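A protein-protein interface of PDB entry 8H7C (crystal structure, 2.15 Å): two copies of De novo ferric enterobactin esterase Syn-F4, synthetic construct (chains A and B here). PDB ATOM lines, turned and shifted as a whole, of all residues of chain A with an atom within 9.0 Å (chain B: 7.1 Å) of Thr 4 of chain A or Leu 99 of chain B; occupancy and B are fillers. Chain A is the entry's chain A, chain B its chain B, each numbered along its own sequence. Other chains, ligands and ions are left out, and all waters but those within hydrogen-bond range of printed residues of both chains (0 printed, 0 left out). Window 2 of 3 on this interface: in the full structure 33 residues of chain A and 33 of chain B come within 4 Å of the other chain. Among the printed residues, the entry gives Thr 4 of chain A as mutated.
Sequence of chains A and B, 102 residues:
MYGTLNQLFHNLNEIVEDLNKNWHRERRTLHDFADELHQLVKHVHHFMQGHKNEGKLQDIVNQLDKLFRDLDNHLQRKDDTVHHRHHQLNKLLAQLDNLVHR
Leu 99 of chain B touches Thr 4 of chain A (CD1 to CG2, 3.3 Å). Leu 5 of chain A touches Leu 5 of chain B. Leu 99 of chain B touches Leu 5 of chain A. Gln 95 of chain B touches Gln 7 of chain A. Leu 8 of chain A touches Gln 95 of chain B. Leu 8 of chain A touches Leu 96 of chain B (CD1 to CA, 3.96 Å). CD1 of Leu 8 of chain A touches CD2 of Leu 99 of chain B (3.7 Å).
Hydrophobic or aromatic side chains of chain B within 4 Å of the printed part of chain A: Leu 5 and Leu 99. Among the printed residues, 7 pairs touch across the chains. Among the printed residues, no Asp or Glu carboxylate lies within 4 Å of a Lys or Arg side-chain nitrogen of the other chain.
The side-chain hydroxyl (OG1) of Thr 4 of chain A sits at hydrogen-bond distance from the side-chain amide oxygen (OE1) of Gln 7 of chain A, 3.0 Å away. O of Gln 7 of chain A sits close to OD1 of Asn 11 of chain A, at 3.0 Å.
Leu 99 of chain B touches just these residues of chain A: Thr 4, Leu 5 and Leu 8. No residue of chain A comes within 4 Å of Val 100 of chain B. Of the printed residues of chain A, Leu 96 of chain B touches Leu 8 (3.96 Å). Of the printed residues of chain A, Leu 5 of chain B touches Leu 5. Printed residues of chain A within 4 Å of Gln 95 of chain B: Gln 7 and Leu 8. Of the printed residues of chain B, Leu 8 of chain A touches Gln 95, Leu 96 and Leu 99. Of the printed residues of chain B, Leu 5 of chain A touches Leu 5 and Leu 99.
Leu 5 of chain A touches its own counterpart, Leu 5 of chain B. Positions printed for both chains: 5, 96 and 100. Of the 7 pairs that touch across the chains among the printed residues, 1 has its exchanged pair printed and touching as well.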
ATOM      1  N   GLY A   3     -16.277  29.573 -35.357  1.00  0.00           N
ATOM      2  CA  GLY A   3     -15.385  28.432 -34.983  1.00  0.00           C
ATOM      3  C   GLY A   3     -16.156  27.158 -34.690  1.00  0.00           C
ATOM      4  O   GLY A   3     -17.388  27.164 -34.632  1.00  0.00           O
ATOM      5  N   THR A   4     -15.426  26.061 -34.520  1.00  0.00           N
ATOM      6  CA  THR A   4     -16.026  24.790 -34.081  1.00  0.00           C
ATOM      7  C   THR A   4     -16.365  24.782 -32.568  1.00  0.00           C
ATOM      8  O   THR A   4     -16.980  23.846 -32.082  1.00  0.00           O
ATOM      9  CB  THR A   4     -15.176  23.552 -34.482  1.00  0.00           C
ATOM     10  OG1 THR A   4     -15.884  22.344 -34.165  1.00  0.00           O
ATOM     11  CG2 THR A   4     -13.850  23.528 -33.778  1.00  0.00           C
ATOM     12  N   LEU A   5     -15.937  25.799 -31.834  1.00  0.00           N
ATOM     13  CA  LEU A   5     -16.436  26.036 -30.491  1.00  0.00           C
ATOM     14  C   LEU A   5     -17.868  26.581 -30.524  1.00  0.00           C
ATOM     15  O   LEU A   5     -18.635  26.352 -29.598  1.00  0.00           O
ATOM     16  CB  LEU A   5     -15.506  26.999 -29.732  1.00  0.00           C
ATOM     17  CG  LEU A   5     -15.492  26.969 -28.197  1.00  0.00           C
ATOM     18  CD1 LEU A   5     -15.138  25.599 -27.623  1.00  0.00           C
ATOM     19  CD2 LEU A   5     -14.515  28.017 -27.686  1.00  0.00           C
ATOM     20  N   ASN A   6     -18.220  27.304 -31.584  1.00  0.00           N
ATOM     21  CA  ASN A   6     -19.589  27.823 -31.754  1.00  0.00           C
ATOM     22  C   ASN A   6     -20.620  26.707 -31.829  1.00  0.00           C
ATOM     23  O   ASN A   6     -21.691  26.813 -31.248  1.00  0.00           O
ATOM     24  CB  ASN A   6     -19.728  28.672 -33.020  1.00  0.00           C
ATOM     25  CG  ASN A   6     -18.896  29.936 -32.981  1.00  0.00           C
ATOM     26  OD1 ASN A   6     -17.659  29.884 -32.948  1.00  0.00           O
ATOM     27  ND2 ASN A   6     -19.566  31.088 -33.005  1.00  0.00           N
ATOM     28  N   GLN A   7     -20.297  25.657 -32.579  1.00  0.00           N
ATOM     29  CA  GLN A   7     -21.170  24.490 -32.675  1.00  0.00           C
ATOM     30  C   GLN A   7     -21.261  23.711 -31.349  1.00  0.00           C
ATOM     31  O   GLN A   7     -22.341  23.250 -30.988  1.00  0.00           O
ATOM     32  CB  GLN A   7     -20.773  23.590 -33.849  1.00  0.00           C
ATOM     33  CG  GLN A   7     -19.420  22.905 -33.725  1.00  0.00           C
ATOM     34  CD  GLN A   7     -19.070  21.972 -34.887  1.00  0.00           C
ATOM     35  OE1 GLN A   7     -18.471  20.913 -34.669  1.00  0.00           O
ATOM     36  NE2 GLN A   7     -19.416  22.362 -36.121  1.00  0.00           N
ATOM     37  N   LEU A   8     -20.139  23.597 -30.626  1.00  0.00           N
ATOM     38  CA  LEU A   8     -20.109  22.902 -29.328  1.00  0.00           C
ATOM     39  C   LEU A   8     -20.948  23.626 -28.301  1.00  0.00           C
ATOM     40  O   LEU A   8     -21.722  22.998 -27.597  1.00  0.00           O
ATOM     41  CB  LEU A   8     -18.689  22.758 -28.769  1.00  0.00           C
ATOM     42  CG  LEU A   8     -17.647  21.965 -29.559  1.00  0.00           C
ATOM     43  CD1 LEU A   8     -16.367  21.870 -28.739  1.00  0.00           C
ATOM     44  CD2 LEU A   8     -18.110  20.579 -29.976  1.00  0.00           C
ATOM     45  N   PHE A   9     -20.756  24.934 -28.200  1.00  0.00           N
ATOM     46  CA  PHE A   9     -21.606  25.763 -27.371  1.00  0.00           C
ATOM     47  C   PHE A   9     -23.087  25.604 -27.710  1.00  0.00           C
ATOM     48  O   PHE A   9     -23.931  25.517 -26.823  1.00  0.00           O
ATOM     49  CB  PHE A   9     -21.275  27.231 -27.528  1.00  0.00           C
ATOM     50  CG  PHE A   9     -22.257  28.117 -26.839  1.00  0.00           C
ATOM     51  CD1 PHE A   9     -22.388  28.066 -25.460  1.00  0.00           C
ATOM     52  CD2 PHE A   9     -23.086  28.957 -27.556  1.00  0.00           C
ATOM     53  CE1 PHE A   9     -23.296  28.872 -24.801  1.00  0.00           C
ATOM     54  CE2 PHE A   9     -24.017  29.759 -26.904  1.00  0.00           C
ATOM     55  CZ  PHE A   9     -24.122  29.714 -25.523  1.00  0.00           C
ATOM     56  N   HIS A  10     -23.384  25.596 -29.004  1.00  0.00           N
ATOM     57  CA  HIS A  10     -24.758  25.508 -29.498  1.00  0.00           C
ATOM     58  C   HIS A  10     -25.343  24.144 -29.125  1.00  0.00           C
ATOM     59  O   HIS A  10     -26.456  24.065 -28.616  1.00  0.00           O
ATOM     60  CB  HIS A  10     -24.750  25.740 -31.013  1.00  0.00           C
ATOM     61  CG  HIS A  10     -26.045  25.451 -31.693  1.00  0.00           C
ATOM     62  ND1 HIS A  10     -26.422  24.176 -32.058  1.00  0.00           N
ATOM     63  CD2 HIS A  10     -27.016  26.275 -32.140  1.00  0.00           C
ATOM     64  CE1 HIS A  10     -27.589  24.227 -32.672  1.00  0.00           C
ATOM     65  NE2 HIS A  10     -27.970  25.489 -32.736  1.00  0.00           N
ATOM     66  N   ASN A  11     -24.570  23.087 -29.355  1.00  0.00           N
ATOM     67  CA  ASN A  11     -24.961  21.740 -28.972  1.00  0.00           C
ATOM     68  C   ASN A  11     -25.229  21.599 -27.477  1.00  0.00           C
ATOM     69  O   ASN A  11     -26.280  21.101 -27.093  1.00  0.00           O
ATOM     70  CB  ASN A  11     -23.888  20.736 -29.407  1.00  0.00           C
ATOM     71  CG  ASN A  11     -23.813  20.577 -30.927  1.00  0.00           C
ATOM     72  OD1 ASN A  11     -24.499  21.272 -31.671  1.00  0.00           O
ATOM     73  ND2 ASN A  11     -22.992  19.651 -31.383  1.00  0.00           N
ATOM     74  N   LEU A  96     -18.604  29.329 -21.472  1.00  0.00           N
ATOM     75  CA  LEU A  96     -18.356  28.865 -22.824  1.00  0.00           C
ATOM     76  C   LEU A  96     -18.835  29.904 -23.838  1.00  0.00           C
ATOM     77  O   LEU A  96     -18.199  30.119 -24.862  1.00  0.00           O
ATOM     78  CB  LEU A  96     -19.031  27.505 -23.058  1.00  0.00           C
ATOM     79  CG  LEU A  96     -18.909  26.869 -24.450  1.00  0.00           C
ATOM     80  CD1 LEU A  96     -17.478  26.884 -24.983  1.00  0.00           C
ATOM     81  CD2 LEU A  96     -19.447  25.441 -24.427  1.00  0.00           C
ATOM     82  N   VAL A 100     -16.722  31.916 -26.880  1.00  0.00           N
ATOM     83  CA  VAL A 100     -17.252  32.016 -28.245  1.00  0.00           C
ATOM     84  C   VAL A 100     -17.397  33.485 -28.684  1.00  0.00           C
ATOM     85  O   VAL A 100     -16.935  33.829 -29.759  1.00  0.00           O
ATOM     86  CB  VAL A 100     -18.599  31.238 -28.387  1.00  0.00           C
ATOM     87  CG1 VAL A 100     -19.294  31.511 -29.719  1.00  0.00           C
ATOM     88  CG2 VAL A 100     -18.358  29.739 -28.241  1.00  0.00           C
ATOM     89  N   LEU B   5     -10.109  26.646 -22.093  1.00  0.00           N
ATOM     90  CA  LEU B   5     -10.754  25.481 -22.685  1.00  0.00           C
ATOM     91  C   LEU B   5     -10.506  24.192 -21.882  1.00  0.00           C
ATOM     92  O   LEU B   5     -11.425  23.391 -21.683  1.00  0.00           O
ATOM     93  CB  LEU B   5     -10.309  25.310 -24.151  1.00  0.00           C
ATOM     94  CG  LEU B   5     -11.396  24.845 -25.126  1.00  0.00           C
ATOM     95  CD1 LEU B   5     -12.636  25.730 -25.081  1.00  0.00           C
ATOM     96  CD2 LEU B   5     -10.841  24.803 -26.539  1.00  0.00           C
ATOM     97  N   LEU B  93     -17.892  15.880 -25.275  1.00  0.00           N
ATOM     98  CA  LEU B  93     -16.635  15.866 -24.523  1.00  0.00           C
ATOM     99  C   LEU B  93     -15.481  15.502 -25.433  1.00  0.00           C
ATOM    100  O   LEU B  93     -14.434  16.125 -25.358  1.00  0.00           O
ATOM    101  CB  LEU B  93     -16.669  14.864 -23.373  1.00  0.00           C
ATOM    102  CG  LEU B  93     -17.264  15.322 -22.047  1.00  0.00           C
ATOM    103  CD1 LEU B  93     -17.144  14.170 -21.062  1.00  0.00           C
ATOM    104  CD2 LEU B  93     -16.588  16.568 -21.493  1.00  0.00           C
ATOM    105  N   ALA B  94     -15.690  14.503 -26.292  1.00  0.00           N
ATOM    106  CA  ALA B  94     -14.661  14.045 -27.213  1.00  0.00           C
ATOM    107  C   ALA B  94     -14.322  15.143 -28.212  1.00  0.00           C
ATOM    108  O   ALA B  94     -13.155  15.421 -28.436  1.00  0.00           O
ATOM    109  CB  ALA B  94     -15.105  12.795 -27.922  1.00  0.00           C
ATOM    110  N   GLN B  95     -15.333  15.789 -28.785  1.00  0.00           N
ATOM    111  CA  GLN B  95     -15.088  16.926 -29.679  1.00  0.00           C
ATOM    112  C   GLN B  95     -14.370  18.062 -28.943  1.00  0.00           C
ATOM    113  O   GLN B  95     -13.525  18.749 -29.511  1.00  0.00           O
ATOM    114  CB  GLN B  95     -16.393  17.423 -30.324  1.00  0.00           C
ATOM    115  CG  GLN B  95     -17.059  16.414 -31.269  1.00  0.00           C
ATOM    116  CD  GLN B  95     -18.309  16.959 -31.964  1.00  0.00           C
ATOM    117  OE1 GLN B  95     -18.227  17.927 -32.723  1.00  0.00           O
ATOM    118  NE2 GLN B  95     -19.464  16.334 -31.720  1.00  0.00           N
ATOM    119  N   LEU B  96     -14.689  18.234 -27.666  1.00  0.00           N
ATOM    120  CA  LEU B  96     -14.063  19.268 -26.843  1.00  0.00           C
ATOM    121  C   LEU B  96     -12.600  18.918 -26.542  1.00  0.00           C
ATOM    122  O   LEU B  96     -11.721  19.742 -26.734  1.00  0.00           O
ATOM    123  CB  LEU B  96     -14.841  19.465 -25.538  1.00  0.00           C
ATOM    124  CG  LEU B  96     -14.965  20.878 -24.986  1.00  0.00           C
ATOM    125  CD1 LEU B  96     -15.380  20.787 -23.528  1.00  0.00           C
ATOM    126  CD2 LEU B  96     -13.695  21.700 -25.110  1.00  0.00           C
ATOM    127  N   ASP B  97     -12.381  17.701 -26.048  1.00  0.00           N
ATOM    128  CA  ASP B  97     -11.058  17.070 -25.867  1.00  0.00           C
ATOM    129  C   ASP B  97     -10.126  17.351 -27.058  1.00  0.00           C
ATOM    130  O   ASP B  97      -9.050  17.919 -26.905  1.00  0.00           O
ATOM    131  CB  ASP B  97     -11.266  15.548 -25.696  1.00  0.00           C
ATOM    132  CG  ASP B  97     -10.065  14.826 -25.125  1.00  0.00           C
ATOM    133  OD1 ASP B  97      -9.134  15.469 -24.598  1.00  0.00           O
ATOM    134  OD2 ASP B  97     -10.075  13.579 -25.194  1.00  0.00           O
ATOM    135  N   ASN B  98     -10.599  17.004 -28.246  1.00  0.00           N
ATOM    136  CA  ASN B  98      -9.901  17.254 -29.510  1.00  0.00           C
ATOM    137  C   ASN B  98      -9.506  18.727 -29.712  1.00  0.00           C
ATOM    138  O   ASN B  98      -8.502  19.028 -30.353  1.00  0.00           O
ATOM    139  CB  ASN B  98     -10.795  16.791 -30.674  1.00  0.00           C
ATOM    140  CG  ASN B  98     -10.027  16.552 -31.963  1.00  0.00           C
ATOM    141  OD1 ASN B  98      -8.947  15.951 -31.963  1.00  0.00           O
ATOM    142  ND2 ASN B  98     -10.601  16.991 -33.081  1.00  0.00           N
ATOM    143  N   LEU B  99     -10.304  19.627 -29.151  1.00  0.00           N
ATOM    144  CA  LEU B  99     -10.096  21.077 -29.248  1.00  0.00           C
ATOM    145  C   LEU B  99      -9.101  21.677 -28.246  1.00  0.00           C
ATOM    146  O   LEU B  99      -8.435  22.651 -28.570  1.00  0.00           O
ATOM    147  CB  LEU B  99     -11.447  21.793 -29.123  1.00  0.00           C
ATOM    148  CG  LEU B  99     -11.834  22.755 -30.235  1.00  0.00           C
ATOM    149  CD1 LEU B  99     -11.893  22.037 -31.571  1.00  0.00           C
ATOM    150  CD2 LEU B  99     -13.181  23.376 -29.900  1.00  0.00           C
ATOM    151  N   VAL B 100      -9.000  21.113 -27.046  1.00  0.00           N
ATOM    152  CA  VAL B 100      -8.064  21.646 -26.034  1.00  0.00           C
ATOM    153  C   VAL B 100      -6.595  21.258 -26.323  1.00  0.00           C
ATOM    154  O   VAL B 100      -5.672  22.003 -25.966  1.00  0.00           O
ATOM    155  CB  VAL B 100      -8.445  21.296 -24.560  1.00  0.00           C
ATOM    156  CG1 VAL B 100      -9.934  21.483 -24.304  1.00  0.00           C
ATOM    157  CG2 VAL B 100      -7.997  19.895 -24.162  1.00  0.00           C
ATOM    158  N   HIS B 101      -6.384  20.104 -26.963  1.00  0.00           N
ATOM    159  CA  HIS B 101      -5.026  19.574 -27.216  1.00  0.00           C
ATOM    160  C   HIS B 101      -4.574  19.793 -28.668  1.00  0.00           C
ATOM    161  O   HIS B 101      -3.758  19.033 -29.192  1.00  0.00           O
ATOM    162  CB  HIS B 101      -4.953  18.081 -26.845  1.00  0.00           C
ATOM    163  CG  HIS B 101      -5.328  17.794 -25.425  1.00  0.00           C
ATOM    164  ND1 HIS B 101      -6.485  17.132 -25.080  1.00  0.00           N
ATOM    165  CD2 HIS B 101      -4.713  18.108 -24.262  1.00  0.00           C
ATOM    166  CE1 HIS B 101      -6.559  17.039 -23.763  1.00  0.00           C
ATOM    167  NE2 HIS B 101      -5.500  17.630 -23.242  1.00  0.00           N
ATOM    168  N   ARG B 102      -5.068  20.857 -29.294  1.00  0.00           N
ATOM    169  CA  ARG B 102      -4.885  21.088 -30.726  1.00  0.00           C
ATOM    170  C   ARG B 102      -3.916  22.236 -30.995  1.00  0.00           C
ATOM    171  O   ARG B 102      -3.187  22.223 -31.986  1.00  0.00           O
ATOM    172  CB  ARG B 102      -6.235  21.415 -31.355  1.00  0.00           C
ATOM    173  CG  ARG B 102      -6.302  21.198 -32.852  1.00  0.00           C
ATOM    174  CD  ARG B 102      -6.440  19.725 -33.204  1.00  0.00           C
ATOM    175  NE  ARG B 102      -6.865  19.556 -34.594  1.00  0.00           N
ATOM    176  CZ  ARG B 102      -7.307  18.420 -35.136  1.00  0.00           C
ATOM    177  NH1 ARG B 102      -7.398  17.297 -34.420  1.00  0.00           N
ATOM    178  NH2 ARG B 102      -7.665  18.406 -36.419  1.00  0.00           N
ATOM    179  OXT ARG B 102      -3.856  23.213 -30.248  1.00  0.00           O
